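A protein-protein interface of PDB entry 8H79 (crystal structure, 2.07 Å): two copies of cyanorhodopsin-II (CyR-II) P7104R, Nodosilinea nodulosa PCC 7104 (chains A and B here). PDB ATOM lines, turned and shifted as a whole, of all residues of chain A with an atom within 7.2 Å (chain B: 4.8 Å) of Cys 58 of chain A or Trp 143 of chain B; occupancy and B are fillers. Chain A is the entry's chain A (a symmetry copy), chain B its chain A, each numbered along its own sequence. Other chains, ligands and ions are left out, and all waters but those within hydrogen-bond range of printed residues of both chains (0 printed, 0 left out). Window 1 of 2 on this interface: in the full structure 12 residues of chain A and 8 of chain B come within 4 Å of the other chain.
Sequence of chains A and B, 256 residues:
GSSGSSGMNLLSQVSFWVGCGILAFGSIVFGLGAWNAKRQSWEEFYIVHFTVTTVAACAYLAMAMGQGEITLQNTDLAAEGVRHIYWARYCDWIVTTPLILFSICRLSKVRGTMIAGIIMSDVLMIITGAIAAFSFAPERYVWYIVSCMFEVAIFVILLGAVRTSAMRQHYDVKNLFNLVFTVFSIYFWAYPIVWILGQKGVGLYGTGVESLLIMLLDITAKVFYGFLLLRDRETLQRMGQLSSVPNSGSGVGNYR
NE1 of Trp 143 of chain B sits close to NE2 of Gln 67 of chain A.
The side-chain amide oxygen (OE1) of Gln 67 of chain A sits at hydrogen-bond distance from the side-chain hydroxyl (OG) of Ser 135 of chain B (3.0 Å).
The side-chain hydroxyl (OG) of Ser 135 of chain B is in hydrogen-bond range of the backbone carbonyl oxygen (O) of Ile 131 of chain B (2.7 Å).
The side-chain sulfur (SG) of Cys 58 of chain A is in hydrogen-bond range of the backbone carbonyl oxygen (O) of Thr 54 of chain A (3.4 Å).
N of Gln 67 of chain A lies within hydrogen-bond range of O of Ala 62 of chain A (2.8 Å).
The backbone carbonyl oxygen of Ser 135 of chain B is in hydrogen-bond range of the guanidinium group of Arg 140 of chain B (2.8 Å).
Among the printed residues, merely in contact across the chains: Thr 54 of chain A with Phe 150 of chain B (3.5 Å), Cys 58 of chain A with Trp 143 of chain B (3.3 Å), Leu 61 of chain A with Trp 143 of chain B (3.9 Å), Ala 62 of chain A with Trp 143 of chain B (3.7 Å), Met 65 of chain A with Glu 139 of chain B (3.8 Å), Met 65 of chain A with Trp 143 of chain B (3.2 Å) and Gln 67 of chain A with Glu 139 of chain B (3.9 Å).
Of the printed residues of chain B, Thr 54 of chain A touches Phe 150 (3.5 Å).
Cys 58 of chain A touches just one residue of chain B: Trp 143 (3.3 Å).
Ala 59 of chain A touches none of the printed residues of chain B.
Printed residues of chain B within 4 Å of Leu 61 of chain A: Trp 143 (3.9 Å).
Of the printed residues of chain A, Ser 135 of chain B touches Gln 67 (3.0 Å).
Trp 143 of chain B touches five residues of chain A.
The nearest printed residue of chain A that does not touch Phe 150 of chain B is Cys 58 of chain A (4.2 Å).
Printed residues of chain B that touch a printed residue of chain A: Ser 135, Glu 139, Trp 143 and Phe 150.
Of the 19 printed residues of chain A, 6 touch a printed residue of chain B.
Hydrophobic or aromatic side chains of chain A that line the printed part of chain B: Leu 61, Ala 62 and Met 65.
No position is printed for both chains.
Of the 9 pairs that touch across the chains among the printed residues, none has its exchanged pair printed and touching as well.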
ATOM      1  N   CYS A  20       9.416 -24.500 -29.991  1.00  0.00           N
ATOM      2  CA  CYS A  20       8.186 -25.045 -30.560  1.00  0.00           C
ATOM      3  C   CYS A  20       8.426 -25.626 -31.952  1.00  0.00           C
ATOM      4  O   CYS A  20       8.038 -26.770 -32.241  1.00  0.00           O
ATOM      5  CB  CYS A  20       7.126 -23.949 -30.604  1.00  0.00           C
ATOM      6  SG  CYS A  20       5.508 -24.512 -31.146  1.00  0.00           S
ATOM      7  N   LEU A  23      10.820 -28.775 -31.770  1.00  0.00           N
ATOM      8  CA  LEU A  23      10.050 -29.899 -31.242  1.00  0.00           C
ATOM      9  C   LEU A  23       9.033 -30.407 -32.264  1.00  0.00           C
ATOM     10  O   LEU A  23       8.875 -31.620 -32.440  1.00  0.00           O
ATOM     11  CB  LEU A  23       9.360 -29.491 -29.937  1.00  0.00           C
ATOM     12  CG  LEU A  23      10.332 -29.297 -28.767  1.00  0.00           C
ATOM     13  CD1 LEU A  23       9.733 -28.412 -27.663  1.00  0.00           C
ATOM     14  CD2 LEU A  23      10.789 -30.637 -28.206  1.00  0.00           C
ATOM     15  N   VAL A  52       6.642 -37.581 -26.650  1.00  0.00           N
ATOM     16  CA  VAL A  52       7.620 -36.724 -25.977  1.00  0.00           C
ATOM     17  C   VAL A  52       7.706 -35.360 -26.654  1.00  0.00           C
ATOM     18  O   VAL A  52       7.537 -34.321 -26.006  1.00  0.00           O
ATOM     19  CB  VAL A  52       8.991 -37.418 -25.923  1.00  0.00           C
ATOM     20  CG1 VAL A  52      10.070 -36.446 -25.447  1.00  0.00           C
ATOM     21  CG2 VAL A  52       8.914 -38.635 -24.987  1.00  0.00           C
ATOM     22  N   THR A  53       7.959 -35.340 -27.971  1.00  0.00           N
ATOM     23  CA  THR A  53       8.117 -34.063 -28.665  1.00  0.00           C
ATOM     24  C   THR A  53       6.800 -33.305 -28.757  1.00  0.00           C
ATOM     25  O   THR A  53       6.791 -32.068 -28.681  1.00  0.00           O
ATOM     26  CB  THR A  53       8.692 -34.269 -30.080  1.00  0.00           C
ATOM     27  OG1 THR A  53       7.828 -35.120 -30.847  1.00  0.00           O
ATOM     28  CG2 THR A  53      10.066 -34.897 -30.020  1.00  0.00           C
ATOM     29  N   THR A  54       5.681 -34.021 -28.918  1.00  0.00           N
ATOM     30  CA  THR A  54       4.399 -33.357 -29.147  1.00  0.00           C
ATOM     31  C   THR A  54       3.876 -32.693 -27.877  1.00  0.00           C
ATOM     32  O   THR A  54       3.346 -31.574 -27.926  1.00  0.00           O
ATOM     33  CB  THR A  54       3.391 -34.368 -29.697  1.00  0.00           C
ATOM     34  OG1 THR A  54       3.860 -34.854 -30.961  1.00  0.00           O
ATOM     35  CG2 THR A  54       2.007 -33.742 -29.867  1.00  0.00           C
ATOM     36  N   VAL A  55       4.028 -33.359 -26.729  1.00  0.00           N
ATOM     37  CA  VAL A  55       3.629 -32.758 -25.460  1.00  0.00           C
ATOM     38  C   VAL A  55       4.466 -31.514 -25.178  1.00  0.00           C
ATOM     39  O   VAL A  55       3.942 -30.470 -24.770  1.00  0.00           O
ATOM     40  CB  VAL A  55       3.746 -33.795 -24.326  1.00  0.00           C
ATOM     41  CG1 VAL A  55       3.642 -33.124 -22.973  1.00  0.00           C
ATOM     42  CG2 VAL A  55       2.694 -34.883 -24.479  1.00  0.00           C
ATOM     43  N   ALA A  56       5.781 -31.604 -25.397  1.00  0.00           N
ATOM     44  CA  ALA A  56       6.639 -30.438 -25.210  1.00  0.00           C
ATOM     45  C   ALA A  56       6.308 -29.341 -26.217  1.00  0.00           C
ATOM     46  O   ALA A  56       6.274 -28.159 -25.861  1.00  0.00           O
ATOM     47  CB  ALA A  56       8.110 -30.843 -25.321  1.00  0.00           C
ATOM     48  N   ALA A  57       6.045 -29.711 -27.473  1.00  0.00           N
ATOM     49  CA  ALA A  57       5.718 -28.701 -28.476  1.00  0.00           C
ATOM     50  C   ALA A  57       4.448 -27.944 -28.106  1.00  0.00           C
ATOM     51  O   ALA A  57       4.332 -26.746 -28.383  1.00  0.00           O
ATOM     52  CB  ALA A  57       5.570 -29.344 -29.854  1.00  0.00           C
ATOM     53  N   CYS A  58       3.480 -28.633 -27.491  1.00  0.00           N
ATOM     54  CA  CYS A  58       2.278 -27.967 -27.001  1.00  0.00           C
ATOM     55  C   CYS A  58       2.602 -27.003 -25.865  1.00  0.00           C
ATOM     56  O   CYS A  58       2.084 -25.879 -25.818  1.00  0.00           O
ATOM     57  CB  CYS A  58       1.256 -29.011 -26.542  1.00  0.00           C
ATOM     58  SG  CYS A  58       0.393 -29.830 -27.925  1.00  0.00           S
ATOM     59  N   ALA A  59       3.434 -27.442 -24.917  1.00  0.00           N
ATOM     60  CA  ALA A  59       3.824 -26.569 -23.815  1.00  0.00           C
ATOM     61  C   ALA A  59       4.581 -25.344 -24.316  1.00  0.00           C
ATOM     62  O   ALA A  59       4.343 -24.227 -23.841  1.00  0.00           O
ATOM     63  CB  ALA A  59       4.658 -27.348 -22.800  1.00  0.00           C
ATOM     64  N   TYR A  60       5.490 -25.525 -25.285  1.00  0.00           N
ATOM     65  CA  TYR A  60       6.209 -24.377 -25.843  1.00  0.00           C
ATOM     66  C   TYR A  60       5.283 -23.457 -26.633  1.00  0.00           C
ATOM     67  O   TYR A  60       5.477 -22.232 -26.636  1.00  0.00           O
ATOM     68  CB  TYR A  60       7.384 -24.856 -26.715  1.00  0.00           C
ATOM     69  CG  TYR A  60       8.666 -25.030 -25.917  1.00  0.00           C
ATOM     70  CD1 TYR A  60       8.844 -26.135 -25.088  1.00  0.00           C
ATOM     71  CD2 TYR A  60       9.667 -24.072 -25.955  1.00  0.00           C
ATOM     72  CE1 TYR A  60      10.005 -26.288 -24.321  1.00  0.00           C
ATOM     73  CE2 TYR A  60      10.834 -24.212 -25.205  1.00  0.00           C
ATOM     74  CZ  TYR A  60      10.997 -25.326 -24.389  1.00  0.00           C
ATOM     75  OH  TYR A  60      12.141 -25.483 -23.633  1.00  0.00           O
ATOM     76  N   LEU A  61       4.265 -24.013 -27.300  1.00  0.00           N
ATOM     77  CA  LEU A  61       3.317 -23.152 -28.004  1.00  0.00           C
ATOM     78  C   LEU A  61       2.559 -22.271 -27.020  1.00  0.00           C
ATOM     79  O   LEU A  61       2.379 -21.070 -27.258  1.00  0.00           O
ATOM     80  CB  LEU A  61       2.348 -23.988 -28.833  1.00  0.00           C
ATOM     81  CG  LEU A  61       1.204 -23.190 -29.482  1.00  0.00           C
ATOM     82  CD1 LEU A  61       1.774 -22.129 -30.420  1.00  0.00           C
ATOM     83  CD2 LEU A  61       0.251 -24.100 -30.231  1.00  0.00           C
ATOM     84  N   ALA A  62       2.144 -22.844 -25.886  1.00  0.00           N
ATOM     85  CA  ALA A  62       1.454 -22.057 -24.870  1.00  0.00           C
ATOM     86  C   ALA A  62       2.347 -20.944 -24.326  1.00  0.00           C
ATOM     87  O   ALA A  62       1.921 -19.789 -24.210  1.00  0.00           O
ATOM     88  CB  ALA A  62       0.959 -22.973 -23.744  1.00  0.00           C
ATOM     89  N   MET A  63       3.593 -21.263 -23.984  1.00  0.00           N
ATOM     90  CA  MET A  63       4.477 -20.218 -23.471  1.00  0.00           C
ATOM     91  C   MET A  63       4.791 -19.174 -24.543  1.00  0.00           C
ATOM     92  O   MET A  63       4.813 -17.969 -24.255  1.00  0.00           O
ATOM     93  CB  MET A  63       5.748 -20.852 -22.906  1.00  0.00           C
ATOM     94  CG  MET A  63       5.458 -21.924 -21.854  1.00  0.00           C
ATOM     95  SD  MET A  63       6.902 -22.469 -20.921  1.00  0.00           S
ATOM     96  CE  MET A  63       7.481 -23.736 -22.042  1.00  0.00           C
ATOM     97  N   ALA A  64       5.006 -19.608 -25.786  1.00  0.00           N
ATOM     98  CA  ALA A  64       5.251 -18.658 -26.873  1.00  0.00           C
ATOM     99  C   ALA A  64       4.106 -17.663 -27.019  1.00  0.00           C
ATOM    100  O   ALA A  64       4.329 -16.496 -27.365  1.00  0.00           O
ATOM    101  CB  ALA A  64       5.473 -19.402 -28.192  1.00  0.00           C
ATOM    102  N   MET A  65       2.874 -18.103 -26.762  1.00  0.00           N
ATOM    103  CA  MET A  65       1.700 -17.253 -26.886  1.00  0.00           C
ATOM    104  C   MET A  65       1.384 -16.494 -25.600  1.00  0.00           C
ATOM    105  O   MET A  65       0.340 -15.839 -25.520  1.00  0.00           O
ATOM    106  CB  MET A  65       0.499 -18.099 -27.322  1.00  0.00           C
ATOM    107  CG  MET A  65       0.611 -18.639 -28.754  1.00  0.00           C
ATOM    108  SD  MET A  65      -0.975 -19.170 -29.459  1.00  0.00           S
ATOM    109  CE  MET A  65      -1.508 -20.338 -28.200  1.00  0.00           C
ATOM    110  N   GLN A  67       1.061 -17.788 -22.395  1.00  0.00           N
ATOM    111  CA  GLN A  67       0.267 -18.539 -21.437  1.00  0.00           C
ATOM    112  C   GLN A  67       1.166 -19.423 -20.576  1.00  0.00           C
ATOM    113  O   GLN A  67       2.368 -19.545 -20.808  1.00  0.00           O
ATOM    114  CB  GLN A  67      -0.783 -19.387 -22.160  1.00  0.00           C
ATOM    115  CG  GLN A  67      -1.548 -18.628 -23.239  1.00  0.00           C
ATOM    116  CD  GLN A  67      -2.520 -19.508 -23.981  1.00  0.00           C
ATOM    117  OE1 GLN A  67      -3.739 -19.400 -23.804  1.00  0.00           O
ATOM    118  NE2 GLN A  67      -1.995 -20.383 -24.825  1.00  0.00           N
ATOM    119  N   ALA A  88       3.738 -24.419 -17.039  1.00  0.00           N
ATOM    120  CA  ALA A  88       3.558 -25.326 -18.171  1.00  0.00           C
ATOM    121  C   ALA A  88       4.728 -26.295 -18.308  1.00  0.00           C
ATOM    122  O   ALA A  88       4.555 -27.403 -18.835  1.00  0.00           O
ATOM    123  CB  ALA A  88       3.382 -24.527 -19.464  1.00  0.00           C
ATOM    124  N   ASP A  92       4.504 -30.456 -18.744  1.00  0.00           N
ATOM    125  CA  ASP A  92       5.247 -31.132 -19.806  1.00  0.00           C
ATOM    126  C   ASP A  92       6.169 -32.199 -19.223  1.00  0.00           C
ATOM    127  O   ASP A  92       6.129 -33.365 -19.635  1.00  0.00           O
ATOM    128  CB  ASP A  92       6.001 -30.057 -20.617  1.00  0.00           C
ATOM    129  CG  ASP A  92       7.159 -30.592 -21.465  1.00  0.00           C
ATOM    130  OD1 ASP A  92       7.348 -31.817 -21.623  1.00  0.00           O
ATOM    131  OD2 ASP A  92       7.894 -29.735 -22.018  1.00  0.00           O
ATOM    132  N   THR B 128      -5.892 -30.130 -24.845  1.00  0.00           N
ATOM    133  CA  THR B 128      -5.876 -28.908 -25.644  1.00  0.00           C
ATOM    134  C   THR B 128      -7.275 -28.319 -25.792  1.00  0.00           C
ATOM    135  O   THR B 128      -7.419 -27.098 -25.905  1.00  0.00           O
ATOM    136  CB  THR B 128      -5.234 -29.178 -27.005  1.00  0.00           C
ATOM    137  OG1 THR B 128      -5.836 -30.331 -27.603  1.00  0.00           O
ATOM    138  CG2 THR B 128      -3.734 -29.454 -26.815  1.00  0.00           C
ATOM    139  N   ILE B 131      -7.589 -26.274 -22.629  1.00  0.00           N
ATOM    140  CA  ILE B 131      -6.812 -25.046 -22.822  1.00  0.00           C
ATOM    141  C   ILE B 131      -7.579 -24.076 -23.708  1.00  0.00           C
ATOM    142  O   ILE B 131      -7.699 -22.885 -23.399  1.00  0.00           O
ATOM    143  CB  ILE B 131      -5.427 -25.356 -23.416  1.00  0.00           C
ATOM    144  CG1 ILE B 131      -4.590 -26.221 -22.467  1.00  0.00           C
ATOM    145  CG2 ILE B 131      -4.680 -24.047 -23.722  1.00  0.00           C
ATOM    146  CD1 ILE B 131      -3.274 -26.706 -23.129  1.00  0.00           C
ATOM    147  N   ALA B 132      -8.107 -24.574 -24.827  1.00  0.00           N
ATOM    148  CA  ALA B 132      -8.936 -23.745 -25.699  1.00  0.00           C
ATOM    149  C   ALA B 132     -10.047 -23.053 -24.917  1.00  0.00           C
ATOM    150  O   ALA B 132     -10.235 -21.838 -25.028  1.00  0.00           O
ATOM    151  CB  ALA B 132      -9.533 -24.600 -26.823  1.00  0.00           C
ATOM    152  N   SER B 135      -8.879 -20.244 -22.788  1.00  0.00           N
ATOM    153  CA  SER B 135      -8.164 -19.193 -23.508  1.00  0.00           C
ATOM    154  C   SER B 135      -9.117 -18.120 -24.028  1.00  0.00           C
ATOM    155  O   SER B 135     -10.277 -18.389 -24.350  1.00  0.00           O
ATOM    156  CB  SER B 135      -7.398 -19.775 -24.702  1.00  0.00           C
ATOM    157  OG  SER B 135      -6.384 -20.676 -24.293  1.00  0.00           O
ATOM    158  N   GLU B 139      -6.134 -17.066 -29.124  1.00  0.00           N
ATOM    159  CA  GLU B 139      -5.514 -18.309 -28.664  1.00  0.00           C
ATOM    160  C   GLU B 139      -6.519 -19.451 -28.634  1.00  0.00           C
ATOM    161  O   GLU B 139      -6.204 -20.578 -29.038  1.00  0.00           O
ATOM    162  CB  GLU B 139      -4.902 -18.108 -27.276  1.00  0.00           C
ATOM    163  CG  GLU B 139      -3.621 -17.267 -27.268  1.00  0.00           C
ATOM    164  CD  GLU B 139      -3.903 -15.776 -27.204  1.00  0.00           C
ATOM    165  OE1 GLU B 139      -5.070 -15.386 -26.950  1.00  0.00           O
ATOM    166  OE2 GLU B 139      -2.956 -14.994 -27.403  1.00  0.00           O
ATOM    167  N   ARG B 140      -7.739 -19.175 -28.155  1.00  0.00           N
ATOM    168  CA  ARG B 140      -8.779 -20.196 -28.126  1.00  0.00           C
ATOM    169  C   ARG B 140      -8.942 -20.870 -29.484  1.00  0.00           C
ATOM    170  O   ARG B 140      -9.105 -22.091 -29.561  1.00  0.00           O
ATOM    171  CB  ARG B 140     -10.104 -19.576 -27.674  1.00  0.00           C
ATOM    172  CG  ARG B 140     -11.297 -20.512 -27.804  1.00  0.00           C
ATOM    173  CD  ARG B 140     -12.404 -20.165 -26.811  1.00  0.00           C
ATOM    174  NE  ARG B 140     -13.281 -19.113 -27.311  1.00  0.00           N
ATOM    175  CZ  ARG B 140     -13.260 -17.856 -26.893  1.00  0.00           C
ATOM    176  NH1 ARG B 140     -12.415 -17.449 -25.957  1.00  0.00           N
ATOM    177  NH2 ARG B 140     -14.115 -16.984 -27.424  1.00  0.00           N
ATOM    178  N   TYR B 141      -8.873 -20.094 -30.569  1.00  0.00           N
ATOM    179  CA  TYR B 141      -9.068 -20.677 -31.898  1.00  0.00           C
ATOM    180  C   TYR B 141      -7.859 -21.495 -32.333  1.00  0.00           C
ATOM    181  O   TYR B 141      -8.014 -22.525 -33.000  1.00  0.00           O
ATOM    182  CB  TYR B 141      -9.377 -19.578 -32.922  1.00  0.00           C
ATOM    183  CG  TYR B 141     -10.511 -18.665 -32.498  1.00  0.00           C
ATOM    184  CD1 TYR B 141     -11.593 -19.161 -31.780  1.00  0.00           C
ATOM    185  CD2 TYR B 141     -10.499 -17.306 -32.813  1.00  0.00           C
ATOM    186  CE1 TYR B 141     -12.630 -18.335 -31.381  1.00  0.00           C
ATOM    187  CE2 TYR B 141     -11.538 -16.472 -32.422  1.00  0.00           C
ATOM    188  CZ  TYR B 141     -12.597 -16.996 -31.699  1.00  0.00           C
ATOM    189  OH  TYR B 141     -13.633 -16.185 -31.301  1.00  0.00           O
ATOM    190  N   VAL B 142      -6.649 -21.053 -31.978  1.00  0.00           N
ATOM    191  CA  VAL B 142      -5.456 -21.849 -32.273  1.00  0.00           C
ATOM    192  C   VAL B 142      -5.545 -23.207 -31.585  1.00  0.00           C
ATOM    193  O   VAL B 142      -5.314 -24.259 -32.200  1.00  0.00           O
ATOM    194  CB  VAL B 142      -4.185 -21.089 -31.847  1.00  0.00           C
ATOM    195  CG1 VAL B 142      -2.948 -22.006 -31.956  1.00  0.00           C
ATOM    196  CG2 VAL B 142      -4.012 -19.824 -32.676  1.00  0.00           C
ATOM    197  N   TRP B 143      -5.863 -23.206 -30.289  1.00  0.00           N
ATOM    198  CA  TRP B 143      -5.966 -24.467 -29.563  1.00  0.00           C
ATOM    199  C   TRP B 143      -7.125 -25.323 -30.067  1.00  0.00           C
ATOM    200  O   TRP B 143      -7.019 -26.554 -30.077  1.00  0.00           O
ATOM    201  CB  TRP B 143      -6.103 -24.187 -28.064  1.00  0.00           C
ATOM    202  CG  TRP B 143      -4.813 -23.736 -27.457  1.00  0.00           C
ATOM    203  CD1 TRP B 143      -4.539 -22.512 -26.929  1.00  0.00           C
ATOM    204  CD2 TRP B 143      -3.603 -24.506 -27.349  1.00  0.00           C
ATOM    205  NE1 TRP B 143      -3.236 -22.473 -26.481  1.00  0.00           N
ATOM    206  CE2 TRP B 143      -2.641 -23.684 -26.727  1.00  0.00           C
ATOM    207  CE3 TRP B 143      -3.250 -25.816 -27.704  1.00  0.00           C
ATOM    208  CZ2 TRP B 143      -1.342 -24.126 -26.448  1.00  0.00           C
ATOM    209  CZ3 TRP B 143      -1.963 -26.254 -27.437  1.00  0.00           C
ATOM    210  CH2 TRP B 143      -1.020 -25.407 -26.808  1.00  0.00           C
ATOM    211  N   TYR B 144      -8.235 -24.705 -30.472  1.00  0.00           N
ATOM    212  CA  TYR B 144      -9.340 -25.487 -31.028  1.00  0.00           C
ATOM    213  C   TYR B 144      -8.888 -26.280 -32.253  1.00  0.00           C
ATOM    214  O   TYR B 144      -9.261 -27.448 -32.415  1.00  0.00           O
ATOM    215  CB  TYR B 144     -10.517 -24.569 -31.371  1.00  0.00           C
ATOM    216  CG  TYR B 144     -11.639 -25.252 -32.139  1.00  0.00           C
ATOM    217  CD1 TYR B 144     -12.621 -25.977 -31.476  1.00  0.00           C
ATOM    218  CD2 TYR B 144     -11.712 -25.168 -33.523  1.00  0.00           C
ATOM    219  CE1 TYR B 144     -13.649 -26.603 -32.170  1.00  0.00           C
ATOM    220  CE2 TYR B 144     -12.728 -25.797 -34.228  1.00  0.00           C
ATOM    221  CZ  TYR B 144     -13.696 -26.511 -33.547  1.00  0.00           C
ATOM    222  OH  TYR B 144     -14.712 -27.134 -34.244  1.00  0.00           O
ATOM    223  N   ILE B 145      -8.060 -25.668 -33.110  1.00  0.00           N
ATOM    224  CA  ILE B 145      -7.579 -26.347 -34.311  1.00  0.00           C
ATOM    225  C   ILE B 145      -6.606 -27.463 -33.941  1.00  0.00           C
ATOM    226  O   ILE B 145      -6.653 -28.563 -34.510  1.00  0.00           O
ATOM    227  CB  ILE B 145      -6.936 -25.332 -35.272  1.00  0.00           C
ATOM    228  CG1 ILE B 145      -8.006 -24.438 -35.909  1.00  0.00           C
ATOM    229  CG2 ILE B 145      -6.081 -26.043 -36.343  1.00  0.00           C
ATOM    230  CD1 ILE B 145      -7.436 -23.179 -36.528  1.00  0.00           C
ATOM    231  N   VAL B 146      -5.711 -27.197 -32.989  1.00  0.00           N
ATOM    232  CA  VAL B 146      -4.791 -28.229 -32.508  1.00  0.00           C
ATOM    233  C   VAL B 146      -5.568 -29.417 -31.955  1.00  0.00           C
ATOM    234  O   VAL B 146      -5.255 -30.579 -32.246  1.00  0.00           O
ATOM    235  CB  VAL B 146      -3.835 -27.643 -31.454  1.00  0.00           C
ATOM    236  CG1 VAL B 146      -3.018 -28.763 -30.792  1.00  0.00           C
ATOM    237  CG2 VAL B 146      -2.930 -26.609 -32.090  1.00  0.00           C
ATOM    238  N   SER B 147      -6.596 -29.146 -31.146  1.00  0.00           N
ATOM    239  CA  SER B 147      -7.432 -30.231 -30.641  1.00  0.00           C
ATOM    240  C   SER B 147      -8.081 -31.006 -31.783  1.00  0.00           C
ATOM    241  O   SER B 147      -8.162 -32.242 -31.740  1.00  0.00           O
ATOM    242  CB  SER B 147      -8.498 -29.675 -29.691  1.00  0.00           C
ATOM    243  OG  SER B 147      -9.159 -30.727 -28.989  1.00  0.00           O
ATOM    244  N   PHE B 150      -5.574 -33.483 -33.284  1.00  0.00           N
ATOM    245  CA  PHE B 150      -5.474 -34.697 -32.478  1.00  0.00           C
ATOM    246  C   PHE B 150      -6.660 -35.622 -32.724  1.00  0.00           C
ATOM    247  O   PHE B 150      -6.508 -36.850 -32.698  1.00  0.00           O
ATOM    248  CB  PHE B 150      -5.373 -34.345 -30.994  1.00  0.00           C
ATOM    249  CG  PHE B 150      -3.993 -33.946 -30.566  1.00  0.00           C
ATOM    250  CD1 PHE B 150      -2.939 -34.835 -30.676  1.00  0.00           C
ATOM    251  CD2 PHE B 150      -3.747 -32.675 -30.077  1.00  0.00           C
ATOM    252  CE1 PHE B 150      -1.654 -34.460 -30.295  1.00  0.00           C
ATOM    253  CE2 PHE B 150      -2.476 -32.294 -29.697  1.00  0.00           C
ATOM    254  CZ  PHE B 150      -1.427 -33.190 -29.809  1.00  0.00           C
